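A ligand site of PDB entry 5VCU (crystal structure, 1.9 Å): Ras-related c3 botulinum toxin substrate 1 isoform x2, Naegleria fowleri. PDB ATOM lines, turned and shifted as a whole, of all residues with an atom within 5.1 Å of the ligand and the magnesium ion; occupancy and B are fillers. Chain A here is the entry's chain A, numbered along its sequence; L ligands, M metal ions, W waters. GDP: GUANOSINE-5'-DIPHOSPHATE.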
ATOM      1  N   ASP A  19       2.665  32.714  13.714  1.00  0.00           N
ATOM      2  CA  ASP A  19       3.793  33.557  13.297  1.00  0.00           C
ATOM      3  C   ASP A  19       4.645  32.905  12.216  1.00  0.00           C
ATOM      4  O   ASP A  19       4.732  31.677  12.093  1.00  0.00           O
ATOM      5  CB  ASP A  19       4.715  33.859  14.488  1.00  0.00           C
ATOM      6  CG  ASP A  19       4.078  34.785  15.509  1.00  0.00           C
ATOM      7  OD1 ASP A  19       4.752  35.048  16.528  1.00  0.00           O
ATOM      8  OD2 ASP A  19       2.935  35.246  15.280  1.00  0.00           O
ATOM      9  N   GLY A  20       5.330  33.741  11.439  1.00  0.00           N
ATOM     10  CA  GLY A  20       6.311  33.217  10.501  1.00  0.00           C
ATOM     11  C   GLY A  20       7.350  32.370  11.215  1.00  0.00           C
ATOM     12  O   GLY A  20       7.748  32.658  12.354  1.00  0.00           O
ATOM     13  N   ALA A  21       7.759  31.284  10.559  1.00  0.00           N
ATOM     14  CA  ALA A  21       8.852  30.382  10.933  1.00  0.00           C
ATOM     15  C   ALA A  21       8.513  29.433  12.079  1.00  0.00           C
ATOM     16  O   ALA A  21       9.408  28.711  12.527  1.00  0.00           O
ATOM     17  CB  ALA A  21      10.132  31.141  11.295  1.00  0.00           C
ATOM     18  N   VAL A  22       7.266  29.391  12.568  1.00  0.00           N
ATOM     19  CA  VAL A  22       6.967  28.447  13.644  1.00  0.00           C
ATOM     20  C   VAL A  22       6.845  27.020  13.136  1.00  0.00           C
ATOM     21  O   VAL A  22       6.904  26.079  13.945  1.00  0.00           O
ATOM     22  CB  VAL A  22       5.704  28.837  14.421  1.00  0.00           C
ATOM     23  CG1 VAL A  22       5.849  30.258  15.032  1.00  0.00           C
ATOM     24  CG2 VAL A  22       4.455  28.719  13.533  1.00  0.00           C
ATOM     25  N   GLY A  23       6.684  26.823  11.829  1.00  0.00           N
ATOM     26  CA  GLY A  23       6.637  25.500  11.260  1.00  0.00           C
ATOM     27  C   GLY A  23       5.305  25.114  10.641  1.00  0.00           C
ATOM     28  O   GLY A  23       5.020  23.912  10.525  1.00  0.00           O
ATOM     29  N   LYS A  24       4.498  26.085  10.223  1.00  0.00           N
ATOM     30  CA  LYS A  24       3.185  25.754   9.638  1.00  0.00           C
ATOM     31  C   LYS A  24       3.351  24.924   8.368  1.00  0.00           C
ATOM     32  O   LYS A  24       2.659  23.907   8.178  1.00  0.00           O
ATOM     33  CB  LYS A  24       2.401  27.032   9.340  1.00  0.00           C
ATOM     34  CG  LYS A  24       2.217  27.956  10.554  1.00  0.00           C
ATOM     35  CD  LYS A  24       1.363  29.183  10.218  1.00  0.00           C
ATOM     36  CE  LYS A  24       2.061  30.110   9.212  1.00  0.00           C
ATOM     37  NZ  LYS A  24       3.391  30.595   9.688  1.00  0.00           N
ATOM     38  N   THR A  25       4.221  25.353   7.468  1.00  0.00           N
ATOM     39  CA  THR A  25       4.351  24.632   6.203  1.00  0.00           C
ATOM     40  C   THR A  25       4.938  23.249   6.426  1.00  0.00           C
ATOM     41  O   THR A  25       4.487  22.266   5.811  1.00  0.00           O
ATOM     42  CB  THR A  25       5.205  25.437   5.230  1.00  0.00           C
ATOM     43  OG1 THR A  25       4.556  26.689   4.970  1.00  0.00           O
ATOM     44  CG2 THR A  25       5.364  24.683   3.918  1.00  0.00           C
ATOM     45  N   ALA A  26       5.931  23.130   7.306  1.00  0.00           N
ATOM     46  CA  ALA A  26       6.530  21.825   7.567  1.00  0.00           C
ATOM     47  C   ALA A  26       5.510  20.888   8.205  1.00  0.00           C
ATOM     48  O   ALA A  26       5.458  19.693   7.883  1.00  0.00           O
ATOM     49  CB  ALA A  26       7.771  21.963   8.451  1.00  0.00           C
ATOM     50  N   LEU A  27       4.670  21.425   9.085  1.00  0.00           N
ATOM     51  CA  LEU A  27       3.567  20.659   9.666  1.00  0.00           C
ATOM     52  C   LEU A  27       2.671  20.070   8.574  1.00  0.00           C
ATOM     53  O   LEU A  27       2.336  18.873   8.592  1.00  0.00           O
ATOM     54  CB  LEU A  27       2.747  21.579  10.569  1.00  0.00           C
ATOM     55  CG  LEU A  27       1.708  20.950  11.469  1.00  0.00           C
ATOM     56  CD1 LEU A  27       2.454  20.360  12.659  1.00  0.00           C
ATOM     57  CD2 LEU A  27       0.699  22.010  11.909  1.00  0.00           C
ATOM     58  N   PHE A  36       9.263  14.734   7.068  1.00  0.00           N
ATOM     59  CA  PHE A  36       9.728  16.105   7.201  1.00  0.00           C
ATOM     60  C   PHE A  36      10.284  16.586   5.862  1.00  0.00           C
ATOM     61  O   PHE A  36      10.986  15.832   5.181  1.00  0.00           O
ATOM     62  CB  PHE A  36      10.808  16.167   8.289  1.00  0.00           C
ATOM     63  CG  PHE A  36      11.205  17.569   8.677  1.00  0.00           C
ATOM     64  CD1 PHE A  36      10.296  18.414   9.279  1.00  0.00           C
ATOM     65  CD2 PHE A  36      12.507  18.003   8.477  1.00  0.00           C
ATOM     66  CE1 PHE A  36      10.671  19.703   9.661  1.00  0.00           C
ATOM     67  CE2 PHE A  36      12.889  19.282   8.849  1.00  0.00           C
ATOM     68  CZ  PHE A  36      11.971  20.132   9.441  1.00  0.00           C
ATOM     69  N   VAL A  41      11.320  24.089   0.747  1.00  0.00           N
ATOM     70  CA  VAL A  41      10.061  24.297   1.450  1.00  0.00           C
ATOM     71  C   VAL A  41       9.444  25.598   0.940  1.00  0.00           C
ATOM     72  O   VAL A  41      10.111  26.649   1.018  1.00  0.00           O
ATOM     73  CB  VAL A  41      10.265  24.357   2.969  1.00  0.00           C
ATOM     74  CG1 VAL A  41       8.954  24.655   3.664  1.00  0.00           C
ATOM     75  CG2 VAL A  41      10.873  23.059   3.468  1.00  0.00           C
ATOM     76  N   PRO A  42       8.225  25.587   0.427  1.00  0.00           N
ATOM     77  CA  PRO A  42       7.617  26.845  -0.030  1.00  0.00           C
ATOM     78  C   PRO A  42       7.207  27.710   1.153  1.00  0.00           C
ATOM     79  O   PRO A  42       7.122  27.263   2.304  1.00  0.00           O
ATOM     80  CB  PRO A  42       6.386  26.370  -0.828  1.00  0.00           C
ATOM     81  CG  PRO A  42       5.983  25.078  -0.110  1.00  0.00           C
ATOM     82  CD  PRO A  42       7.301  24.442   0.300  1.00  0.00           C
ATOM     83  N   THR A  43       6.976  29.001   0.870  1.00  0.00           N
ATOM     84  CA  THR A  43       6.426  29.887   1.889  1.00  0.00           C
ATOM     85  C   THR A  43       5.039  29.417   2.323  1.00  0.00           C
ATOM     86  O   THR A  43       4.750  29.317   3.522  1.00  0.00           O
ATOM     87  CB  THR A  43       6.356  31.324   1.361  1.00  0.00           C
ATOM     88  OG1 THR A  43       5.721  31.339   0.066  1.00  0.00           O
ATOM     89  CG2 THR A  43       7.761  31.924   1.234  1.00  0.00           C
ATOM     90  N   VAL A  44       4.167  29.138   1.360  1.00  0.00           N
ATOM     91  CA  VAL A  44       2.807  28.694   1.646  1.00  0.00           C
ATOM     92  C   VAL A  44       2.542  27.456   0.791  1.00  0.00           C
ATOM     93  O   VAL A  44       2.634  27.501  -0.436  1.00  0.00           O
ATOM     94  CB  VAL A  44       1.774  29.805   1.350  1.00  0.00           C
ATOM     95  CG1 VAL A  44       0.359  29.317   1.646  1.00  0.00           C
ATOM     96  CG2 VAL A  44       2.079  31.054   2.185  1.00  0.00           C
ATOM     97  N   ASP A  65      -2.700  26.381   4.110  1.00  0.00           N
ATOM     98  CA  ASP A  65      -1.543  27.060   4.682  1.00  0.00           C
ATOM     99  C   ASP A  65      -1.750  28.574   4.563  1.00  0.00           C
ATOM    100  O   ASP A  65      -2.579  29.047   3.788  1.00  0.00           O
ATOM    101  CB  ASP A  65      -0.281  26.598   3.936  1.00  0.00           C
ATOM    102  CG  ASP A  65       1.029  26.846   4.725  1.00  0.00           C
ATOM    103  OD1 ASP A  65       1.015  27.395   5.852  1.00  0.00           O
ATOM    104  OD2 ASP A  65       2.093  26.457   4.177  1.00  0.00           O
ATOM    105  N   THR A  66      -1.000  29.341   5.373  1.00  0.00           N
ATOM    106  CA  THR A  66      -1.114  30.803   5.339  1.00  0.00           C
ATOM    107  C   THR A  66       0.255  31.446   5.531  1.00  0.00           C
ATOM    108  O   THR A  66       1.169  30.849   6.109  1.00  0.00           O
ATOM    109  CB  THR A  66      -2.044  31.387   6.430  1.00  0.00           C
ATOM    110  OG1 THR A  66      -1.519  31.090   7.739  1.00  0.00           O
ATOM    111  CG2 THR A  66      -3.468  30.839   6.303  1.00  0.00           C
ATOM    112  N   THR A 123       4.653  23.658  18.198  1.00  0.00           N
ATOM    113  CA  THR A 123       5.482  23.018  17.191  1.00  0.00           C
ATOM    114  C   THR A 123       6.930  22.903  17.652  1.00  0.00           C
ATOM    115  O   THR A 123       7.360  23.491  18.647  1.00  0.00           O
ATOM    116  CB  THR A 123       5.450  23.808  15.864  1.00  0.00           C
ATOM    117  OG1 THR A 123       5.989  25.125  16.107  1.00  0.00           O
ATOM    118  CG2 THR A 123       4.033  23.934  15.332  1.00  0.00           C
ATOM    119  N   LYS A 124       7.694  22.103  16.901  1.00  0.00           N
ATOM    120  CA  LYS A 124       9.123  21.911  17.145  1.00  0.00           C
ATOM    121  C   LYS A 124       9.369  21.302  18.523  1.00  0.00           C
ATOM    122  O   LYS A 124      10.309  21.641  19.238  1.00  0.00           O
ATOM    123  CB  LYS A 124       9.890  23.236  16.971  1.00  0.00           C
ATOM    124  CG  LYS A 124       9.559  23.921  15.647  1.00  0.00           C
ATOM    125  CD  LYS A 124      10.478  25.118  15.382  1.00  0.00           C
ATOM    126  CE  LYS A 124      10.198  25.766  14.019  1.00  0.00           C
ATOM    127  NZ  LYS A 124      11.225  26.832  13.659  1.00  0.00           N
ATOM    128  N   LEU A 125       8.500  20.349  18.890  1.00  0.00           N
ATOM    129  CA  LEU A 125       8.658  19.647  20.161  1.00  0.00           C
ATOM    130  C   LEU A 125      10.028  18.973  20.269  1.00  0.00           C
ATOM    131  O   LEU A 125      10.556  18.819  21.378  1.00  0.00           O
ATOM    132  CB  LEU A 125       7.535  18.630  20.322  1.00  0.00           C
ATOM    133  CG  LEU A 125       7.603  17.720  21.552  1.00  0.00           C
ATOM    134  CD1 LEU A 125       7.628  18.581  22.815  1.00  0.00           C
ATOM    135  CD2 LEU A 125       6.426  16.721  21.600  1.00  0.00           C
ATOM    136  N   ASP A 126      10.604  18.562  19.130  1.00  0.00           N
ATOM    137  CA  ASP A 126      11.921  17.926  19.172  1.00  0.00           C
ATOM    138  C   ASP A 126      12.998  18.894  19.664  1.00  0.00           C
ATOM    139  O   ASP A 126      13.962  18.463  20.301  1.00  0.00           O
ATOM    140  CB  ASP A 126      12.305  17.366  17.801  1.00  0.00           C
ATOM    141  CG  ASP A 126      12.313  18.435  16.703  1.00  0.00           C
ATOM    142  OD1 ASP A 126      11.246  19.033  16.423  1.00  0.00           O
ATOM    143  OD2 ASP A 126      13.400  18.693  16.124  1.00  0.00           O
ATOM    144  N   LEU A 127      12.865  20.185  19.365  1.00  0.00           N
ATOM    145  CA  LEU A 127      13.868  21.131  19.843  1.00  0.00           C
ATOM    146  C   LEU A 127      13.699  21.420  21.333  1.00  0.00           C
ATOM    147  O   LEU A 127      14.693  21.537  22.060  1.00  0.00           O
ATOM    148  CB  LEU A 127      13.795  22.426  19.019  1.00  0.00           C
ATOM    149  CG  LEU A 127      14.048  22.245  17.528  1.00  0.00           C
ATOM    150  CD1 LEU A 127      14.080  23.609  16.826  1.00  0.00           C
ATOM    151  CD2 LEU A 127      15.356  21.490  17.279  1.00  0.00           C
ATOM    152  N   CYS A 165       3.768  19.013  19.301  1.00  0.00           N
ATOM    153  CA  CYS A 165       4.109  18.045  18.265  1.00  0.00           C
ATOM    154  C   CYS A 165       5.398  18.451  17.570  1.00  0.00           C
ATOM    155  O   CYS A 165       5.915  19.549  17.795  1.00  0.00           O
ATOM    156  CB  CYS A 165       2.975  17.902  17.240  1.00  0.00           C
ATOM    157  SG  CYS A 165       2.771  19.349  16.141  1.00  0.00           S
ATOM    158  N   SER A 166       5.929  17.552  16.747  1.00  0.00           N
ATOM    159  CA  SER A 166       7.122  17.809  15.930  1.00  0.00           C
ATOM    160  C   SER A 166       6.895  17.319  14.507  1.00  0.00           C
ATOM    161  O   SER A 166       6.659  16.127  14.287  1.00  0.00           O
ATOM    162  CB  SER A 166       8.375  17.124  16.522  1.00  0.00           C
ATOM    163  OG  SER A 166       9.459  17.144  15.591  1.00  0.00           O
ATOM    164  N   ALA A 167       6.982  18.220  13.530  1.00  0.00           N
ATOM    165  CA  ALA A 167       6.968  17.774  12.146  1.00  0.00           C
ATOM    166  C   ALA A 167       8.230  17.000  11.784  1.00  0.00           C
ATOM    167  O   ALA A 167       8.214  16.230  10.819  1.00  0.00           O
ATOM    168  CB  ALA A 167       6.804  18.954  11.190  1.00  0.00           C
ATOM    169  N   LYS A 168       9.313  17.189  12.540  1.00  0.00           N
ATOM    170  CA  LYS A 168      10.584  16.561  12.198  1.00  0.00           C
ATOM    171  C   LYS A 168      10.618  15.104  12.632  1.00  0.00           C
ATOM    172  O   LYS A 168      11.031  14.217  11.876  1.00  0.00           O
ATOM    173  CB  LYS A 168      11.743  17.326  12.840  1.00  0.00           C
ATOM    174  CG  LYS A 168      13.117  16.779  12.479  1.00  0.00           C
ATOM    175  CD  LYS A 168      14.224  17.732  12.938  1.00  0.00           C
ATOM    176  CE  LYS A 168      15.495  17.525  12.128  1.00  0.00           C
ATOM    177  NZ  LYS A 168      16.598  18.466  12.518  1.00  0.00           N
HETATM  178  PB  GDP L   1       6.343  28.607   8.571  1.00  0.00           P
HETATM  179  O1B GDP L   1       5.485  28.738   9.813  1.00  0.00           O
HETATM  180  O2B GDP L   1       6.907  29.984   8.204  1.00  0.00           O
HETATM  181  O3B GDP L   1       5.578  28.050   7.408  1.00  0.00           O
HETATM  182  O3A GDP L   1       7.557  27.650   8.984  1.00  0.00           O
HETATM  183  PA  GDP L   1       8.276  26.570   8.026  1.00  0.00           P
HETATM  184  O1A GDP L   1       7.438  25.354   7.759  1.00  0.00           O
HETATM  185  O2A GDP L   1       8.778  27.266   6.760  1.00  0.00           O
HETATM  186  O5' GDP L   1       9.541  26.172   8.934  1.00  0.00           O
HETATM  187  C5' GDP L   1      10.475  27.191   9.295  1.00  0.00           C
HETATM  188  C4' GDP L   1      11.770  26.556   9.793  1.00  0.00           C
HETATM  189  O4' GDP L   1      11.516  25.744  10.939  1.00  0.00           O
HETATM  190  C3' GDP L   1      12.412  25.634   8.759  1.00  0.00           C
HETATM  191  O3' GDP L   1      13.824  25.755   8.916  1.00  0.00           O
HETATM  192  C2' GDP L   1      11.966  24.246   9.196  1.00  0.00           C
HETATM  193  O2' GDP L   1      12.861  23.203   8.810  1.00  0.00           O
HETATM  194  C1' GDP L   1      11.938  24.393  10.704  1.00  0.00           C
HETATM  195  N9  GDP L   1      10.955  23.479  11.309  1.00  0.00           N
HETATM  196  C8  GDP L   1       9.628  23.440  11.062  1.00  0.00           C
HETATM  197  N7  GDP L   1       9.038  22.485  11.839  1.00  0.00           N
HETATM  198  C5  GDP L   1      10.002  21.919  12.599  1.00  0.00           C
HETATM  199  C6  GDP L   1      10.062  20.874  13.637  1.00  0.00           C
HETATM  200  O6  GDP L   1       9.031  20.249  13.997  1.00  0.00           O
HETATM  201  N1  GDP L   1      11.267  20.620  14.175  1.00  0.00           N
HETATM  202  C2  GDP L   1      12.399  21.265  13.815  1.00  0.00           C
HETATM  203  N2  GDP L   1      13.566  20.920  14.428  1.00  0.00           N
HETATM  204  N3  GDP L   1      12.417  22.245  12.868  1.00  0.00           N
HETATM  205  C4  GDP L   1      11.257  22.597  12.252  1.00  0.00           C
HETATM  206 MG    MG M   1       5.132  28.644   5.487  1.00  0.00          MG
HETATM  207  O   HOH W   1       9.387  30.374   7.161  1.00  0.00           O
HETATM  208  O   HOH W   2       3.097  29.000   5.952  1.00  0.00           O
HETATM  209  O   HOH W   3      12.226  22.268   6.400  1.00  0.00           O
HETATM  210  O   HOH W   4       5.946  20.756  14.761  1.00  0.00           O
HETATM  211  O   HOH W   5       7.096  28.234   4.975  1.00  0.00           O
HETATM  212  O   HOH W   6      11.069  27.369   5.544  1.00  0.00           O
HETATM  213  O   HOH W   7       5.659  30.625   6.056  1.00  0.00           O
HETATM  214  O   HOH W   8      13.560  25.050  13.452  1.00  0.00           O
HETATM  215  O   HOH W   9       6.236  22.137  12.436  1.00  0.00           O
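O1B of the ligand is in hydrogen-bond range of N of Lys 24, at 2.9 Å.
O1B of the ligand is in hydrogen-bond range of N of Val 22.
N of Ala 21 sits at hydrogen-bond distance from O2B of the ligand, 2.8 Å away.
O6 of the ligand is in hydrogen-bond range of N of Ala 167 (2.9 Å).
N of Ala 26 sits at hydrogen-bond distance from O1A of the ligand (2.7 Å).
N of Gly 23 lies within hydrogen-bond range of O1B of the ligand (3.0 Å).
OD1 of Asp 126 sits at hydrogen-bond distance from N1 of the ligand.
O1B of the ligand lies within salt-bridge range of NZ of Lys 24.
An oxygen (O4') of the ligand lies within hydrogen-bond range of the side-chain amino group (NZ) of Lys 124 (2.9 Å).
The backbone NH (N) of Lys 168 is in hydrogen-bond range of an oxygen (O6) of the ligand, 3.4 Å away.
The backbone NH (N) of Thr 25 lies within hydrogen-bond range of an oxygen (O1A) of the ligand (3.2 Å).
Asp 19 touches the ligand (O to O1B, 3.8 Å).
C of Gly 20 touches O2B of the ligand, at 3.9 Å.
Phe 36 touches the ligand (CZ to O2', 3.3 Å).
Leu 127 touches the ligand (CG to N2, 3.4 Å).
OG of Ser 166 touches O6 of the ligand, 3.5 Å away.
Hydrophobic or aromatic side chains within 4 Å of the ligand: Val 22, Ala 26, Phe 36, Leu 127 and Ala 167.
The magnesium ion is bound by O3B of the ligand (2.1 Å), water W5 (2.1 Å), OG1 of Thr 25 (2.1 Å), O of Thr 43 (2.1 Å), water W2 (2.1 Å) and water W7 (2.1 Å).
The magnesium ion has six donor atoms within binding distance.
Water W5 bridges O2A of the ligand (2.6 Å) and O of Pro 42 (2.8 Å).
Water W2 bridges the side-chain carboxylate (OD1) of Asp 65 (2.6 Å) and the backbone carbonyl oxygen (O) of Thr 66 (2.7 Å).
Water W9 lies within hydrogen-bond range of O of Gly 23 (2.9 Å) and N7 of the ligand (2.9 Å).
Water W8 lies within hydrogen-bond range of the side-chain amino group (NZ) of Lys 124 and a nitrogen (N3) of the ligand.
Water W4 lies within hydrogen-bond range of N of Ala 167, N of Lys 124, O6 of the ligand and O of Cys 165.
The side-chain hydroxyl (OG1) of Thr 25 lies close to the side-chain carboxylate (OD2) of Asp 65, at 2.6 Å.
The backbone NH (N) of Lys 168 sits at hydrogen-bond distance from the side-chain hydroxyl (OG) of Ser 166 (3.1 Å).
N of Lys 124 is in hydrogen-bond range of O of Cys 165, at 3.2 Å.
The side-chain carboxylate (OD1) of Asp 126 sits at hydrogen-bond distance from the side-chain hydroxyl (OG) of Ser 166.
The side-chain amino group of Lys 24 sits at hydrogen-bond distance from the backbone carbonyl oxygen of Asp 19 (3.0 Å).
OG1 of Thr 123 is in hydrogen-bond range of O of Val 22 (2.5 Å).
The side-chain amino group (NZ) of Lys 124 lies within hydrogen-bond range of the backbone carbonyl oxygen (O) of Ala 21.
Merely in contact with the magnesium ion: Pro 42 (3.9998 Å) and Asp 65 (3.97 Å).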
